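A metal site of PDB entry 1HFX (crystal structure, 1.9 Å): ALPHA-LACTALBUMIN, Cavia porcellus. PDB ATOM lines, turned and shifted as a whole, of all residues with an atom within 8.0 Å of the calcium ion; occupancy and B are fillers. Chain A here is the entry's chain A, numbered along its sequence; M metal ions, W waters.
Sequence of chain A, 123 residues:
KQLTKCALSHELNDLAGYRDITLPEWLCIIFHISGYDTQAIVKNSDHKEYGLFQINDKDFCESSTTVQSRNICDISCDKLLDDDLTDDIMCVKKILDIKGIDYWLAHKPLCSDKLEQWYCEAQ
The side-chain carboxylate (OD1) of Asp 84 sits at hydrogen-bond distance from the side-chain hydroxyl (OG1) of Thr 86 (2.6 Å).
Of the 16 residues printed, 5 come within 4 Å of the calcium ion.
Along chain A the residues within 4 Å of the calcium ion span positions 79 to 88.
The nearest printed residue that does not touch the calcium ion is Leu 80 (4.2 Å).
The calcium ion is bound by O of Asp 84 (2.2 Å).
The calcium ion is bound by O of Lys 79.
The calcium ion is bound by water W1 (2.3 Å).
OD1 of Asp 88 is bound to the calcium ion.
The side-chain carboxylate (OD1) of Asp 82 is bound to the calcium ion, at 2.4 Å.
OD1 of Asp 87 binds the calcium ion (2.4 Å).
Water W2 binds the calcium ion.
Water W2 bridges the side-chain carboxylate (OD2) of Asp 82 (2.7 Å) and the side-chain carboxylate (OD2) of Asp 87 (2.8 Å).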
ATOM      1  N   THR A  38      15.491 -27.012  18.728  1.00  0.00           N
ATOM      2  CA  THR A  38      16.357 -26.395  17.730  1.00  0.00           C
ATOM      3  C   THR A  38      15.771 -25.068  17.258  1.00  0.00           C
ATOM      4  O   THR A  38      16.483 -24.227  16.718  1.00  0.00           O
ATOM      5  CB  THR A  38      16.554 -27.277  16.475  1.00  0.00           C
ATOM      6  OG1 THR A  38      15.277 -27.550  15.885  1.00  0.00           O
ATOM      7  CG2 THR A  38      17.267 -28.573  16.814  1.00  0.00           C
ATOM      8  N   ILE A  75      27.153 -16.191   9.511  1.00  0.00           N
ATOM      9  CA  ILE A  75      26.058 -17.100   9.225  1.00  0.00           C
ATOM     10  C   ILE A  75      24.739 -16.407   9.498  1.00  0.00           C
ATOM     11  O   ILE A  75      24.649 -15.556  10.376  1.00  0.00           O
ATOM     12  CB  ILE A  75      26.186 -18.382  10.122  1.00  0.00           C
ATOM     13  CG1 ILE A  75      25.325 -19.523   9.574  1.00  0.00           C
ATOM     14  CG2 ILE A  75      25.847 -18.065  11.590  1.00  0.00           C
ATOM     15  CD1 ILE A  75      25.496 -20.849  10.302  1.00  0.00           C
ATOM     16  N   SER A  76      23.751 -16.661   8.645  1.00  0.00           N
ATOM     17  CA  SER A  76      22.423 -16.088   8.846  1.00  0.00           C
ATOM     18  C   SER A  76      21.804 -16.891   9.981  1.00  0.00           C
ATOM     19  O   SER A  76      21.999 -18.100  10.064  1.00  0.00           O
ATOM     20  CB  SER A  76      21.613 -16.222   7.573  1.00  0.00           C
ATOM     21  OG  SER A  76      22.270 -15.535   6.520  1.00  0.00           O
ATOM     22  N   CYS A  77      21.071 -16.223  10.864  1.00  0.00           N
ATOM     23  CA  CYS A  77      20.464 -16.904  12.008  1.00  0.00           C
ATOM     24  C   CYS A  77      19.454 -17.976  11.667  1.00  0.00           C
ATOM     25  O   CYS A  77      19.251 -18.897  12.454  1.00  0.00           O
ATOM     26  CB  CYS A  77      19.827 -15.894  12.963  1.00  0.00           C
ATOM     27  SG  CYS A  77      20.937 -14.559  13.496  1.00  0.00           S
ATOM     28  N   ASP A  78      18.834 -17.890  10.494  1.00  0.00           N
ATOM     29  CA  ASP A  78      17.838 -18.897  10.127  1.00  0.00           C
ATOM     30  C   ASP A  78      18.456 -20.302  10.003  1.00  0.00           C
ATOM     31  O   ASP A  78      17.788 -21.305  10.204  1.00  0.00           O
ATOM     32  CB  ASP A  78      17.079 -18.496   8.865  1.00  0.00           C
ATOM     33  CG  ASP A  78      17.932 -18.582   7.646  1.00  0.00           C
ATOM     34  OD1 ASP A  78      18.694 -17.644   7.377  1.00  0.00           O
ATOM     35  OD2 ASP A  78      17.846 -19.615   6.945  1.00  0.00           O
ATOM     36  N   LYS A  79      19.755 -20.359   9.705  1.00  0.00           N
ATOM     37  CA  LYS A  79      20.443 -21.636   9.595  1.00  0.00           C
ATOM     38  C   LYS A  79      20.662 -22.273  10.974  1.00  0.00           C
ATOM     39  O   LYS A  79      21.052 -23.443  11.071  1.00  0.00           O
ATOM     40  CB  LYS A  79      21.771 -21.432   8.864  1.00  0.00           C
ATOM     41  CG  LYS A  79      21.577 -21.041   7.414  1.00  0.00           C
ATOM     42  CD  LYS A  79      22.881 -20.957   6.654  1.00  0.00           C
ATOM     43  CE  LYS A  79      23.575 -22.319   6.541  1.00  0.00           C
ATOM     44  NZ  LYS A  79      22.714 -23.395   5.954  1.00  0.00           N
ATOM     45  N   LEU A  80      20.417 -21.506  12.028  1.00  0.00           N
ATOM     46  CA  LEU A  80      20.545 -21.973  13.400  1.00  0.00           C
ATOM     47  C   LEU A  80      19.183 -22.414  13.941  1.00  0.00           C
ATOM     48  O   LEU A  80      19.040 -22.729  15.117  1.00  0.00           O
ATOM     49  CB  LEU A  80      21.122 -20.865  14.293  1.00  0.00           C
ATOM     50  CG  LEU A  80      22.491 -20.324  13.870  1.00  0.00           C
ATOM     51  CD1 LEU A  80      22.847 -19.065  14.676  1.00  0.00           C
ATOM     52  CD2 LEU A  80      23.549 -21.407  14.041  1.00  0.00           C
ATOM     53  N   LEU A  81      18.188 -22.477  13.071  1.00  0.00           N
ATOM     54  CA  LEU A  81      16.854 -22.887  13.486  1.00  0.00           C
ATOM     55  C   LEU A  81      16.405 -24.220  12.872  1.00  0.00           C
ATOM     56  O   LEU A  81      15.353 -24.743  13.218  1.00  0.00           O
ATOM     57  CB  LEU A  81      15.834 -21.795  13.168  1.00  0.00           C
ATOM     58  CG  LEU A  81      16.014 -20.450  13.874  1.00  0.00           C
ATOM     59  CD1 LEU A  81      14.964 -19.493  13.378  1.00  0.00           C
ATOM     60  CD2 LEU A  81      15.935 -20.631  15.380  1.00  0.00           C
ATOM     61  N   ASP A  82      17.188 -24.766  11.955  1.00  0.00           N
ATOM     62  CA  ASP A  82      16.837 -26.053  11.343  1.00  0.00           C
ATOM     63  C   ASP A  82      17.364 -27.234  12.180  1.00  0.00           C
ATOM     64  O   ASP A  82      17.936 -27.025  13.258  1.00  0.00           O
ATOM     65  CB  ASP A  82      17.302 -26.112   9.881  1.00  0.00           C
ATOM     66  CG  ASP A  82      18.792 -25.858   9.722  1.00  0.00           C
ATOM     67  OD1 ASP A  82      19.540 -26.259  10.614  1.00  0.00           O
ATOM     68  OD2 ASP A  82      19.196 -25.213   8.729  1.00  0.00           O
ATOM     69  N   ASP A  83      17.182 -28.455  11.689  1.00  0.00           N
ATOM     70  CA  ASP A  83      17.603 -29.664  12.412  1.00  0.00           C
ATOM     71  C   ASP A  83      19.033 -30.149  12.112  1.00  0.00           C
ATOM     72  O   ASP A  83      19.442 -31.221  12.566  1.00  0.00           O
ATOM     73  CB  ASP A  83      16.588 -30.791  12.199  1.00  0.00           C
ATOM     74  CG  ASP A  83      16.654 -31.400  10.804  1.00  0.00           C
ATOM     75  OD1 ASP A  83      16.483 -30.635   9.817  1.00  0.00           O
ATOM     76  OD2 ASP A  83      16.898 -32.629  10.685  1.00  0.00           O
ATOM     77  N   ASP A  84      19.762 -29.382  11.313  1.00  0.00           N
ATOM     78  CA  ASP A  84      21.149 -29.715  11.021  1.00  0.00           C
ATOM     79  C   ASP A  84      22.002 -28.865  11.936  1.00  0.00           C
ATOM     80  O   ASP A  84      22.107 -27.647  11.759  1.00  0.00           O
ATOM     81  CB  ASP A  84      21.499 -29.457   9.547  1.00  0.00           C
ATOM     82  CG  ASP A  84      22.919 -29.832   9.228  1.00  0.00           C
ATOM     83  OD1 ASP A  84      23.603 -30.377  10.111  1.00  0.00           O
ATOM     84  OD2 ASP A  84      23.362 -29.602   8.093  1.00  0.00           O
ATOM     85  N   LEU A  85      22.605 -29.482  12.937  1.00  0.00           N
ATOM     86  CA  LEU A  85      23.408 -28.758  13.894  1.00  0.00           C
ATOM     87  C   LEU A  85      24.841 -28.556  13.429  1.00  0.00           C
ATOM     88  O   LEU A  85      25.622 -27.916  14.110  1.00  0.00           O
ATOM     89  CB  LEU A  85      23.399 -29.518  15.213  1.00  0.00           C
ATOM     90  CG  LEU A  85      22.275 -29.256  16.236  1.00  0.00           C
ATOM     91  CD1 LEU A  85      20.948 -28.950  15.595  1.00  0.00           C
ATOM     92  CD2 LEU A  85      22.194 -30.449  17.173  1.00  0.00           C
ATOM     93  N   THR A  86      25.170 -29.039  12.238  1.00  0.00           N
ATOM     94  CA  THR A  86      26.539 -28.909  11.707  1.00  0.00           C
ATOM     95  C   THR A  86      27.085 -27.481  11.723  1.00  0.00           C
ATOM     96  O   THR A  86      28.168 -27.233  12.262  1.00  0.00           O
ATOM     97  CB  THR A  86      26.607 -29.523  10.266  1.00  0.00           C
ATOM     98  OG1 THR A  86      26.174 -30.891  10.311  1.00  0.00           O
ATOM     99  CG2 THR A  86      28.020 -29.486   9.707  1.00  0.00           C
ATOM    100  N   ASP A  87      26.362 -26.543  11.113  1.00  0.00           N
ATOM    101  CA  ASP A  87      26.802 -25.149  11.111  1.00  0.00           C
ATOM    102  C   ASP A  87      26.674 -24.496  12.479  1.00  0.00           C
ATOM    103  O   ASP A  87      27.486 -23.651  12.825  1.00  0.00           O
ATOM    104  CB  ASP A  87      26.107 -24.311  10.015  1.00  0.00           C
ATOM    105  CG  ASP A  87      24.603 -24.521   9.953  1.00  0.00           C
ATOM    106  OD1 ASP A  87      23.994 -25.146  10.838  1.00  0.00           O
ATOM    107  OD2 ASP A  87      24.011 -24.059   8.962  1.00  0.00           O
ATOM    108  N   ASP A  88      25.678 -24.912  13.253  1.00  0.00           N
ATOM    109  CA  ASP A  88      25.516 -24.382  14.611  1.00  0.00           C
ATOM    110  C   ASP A  88      26.787 -24.686  15.391  1.00  0.00           C
ATOM    111  O   ASP A  88      27.357 -23.808  16.024  1.00  0.00           O
ATOM    112  CB  ASP A  88      24.360 -25.090  15.330  1.00  0.00           C
ATOM    113  CG  ASP A  88      23.013 -24.871  14.663  1.00  0.00           C
ATOM    114  OD1 ASP A  88      22.877 -25.074  13.453  1.00  0.00           O
ATOM    115  OD2 ASP A  88      22.058 -24.523  15.381  1.00  0.00           O
ATOM    116  N   ILE A  89      27.211 -25.943  15.376  1.00  0.00           N
ATOM    117  CA  ILE A  89      28.402 -26.359  16.095  1.00  0.00           C
ATOM    118  C   ILE A  89      29.633 -25.601  15.585  1.00  0.00           C
ATOM    119  O   ILE A  89      30.492 -25.198  16.387  1.00  0.00           O
ATOM    120  CB  ILE A  89      28.567 -27.882  16.023  1.00  0.00           C
ATOM    121  CG1 ILE A  89      27.492 -28.512  16.909  1.00  0.00           C
ATOM    122  CG2 ILE A  89      29.985 -28.318  16.471  1.00  0.00           C
ATOM    123  CD1 ILE A  89      27.301 -29.982  16.661  1.00  0.00           C
HETATM  124 CA    CA M   1      21.686 -25.546  11.501  1.00  0.00          CA
HETATM  125  O   HOH W   1      20.237 -25.462  13.325  1.00  0.00           O
HETATM  126  O   HOH W   2      21.825 -25.849   9.086  1.00  0.00           O
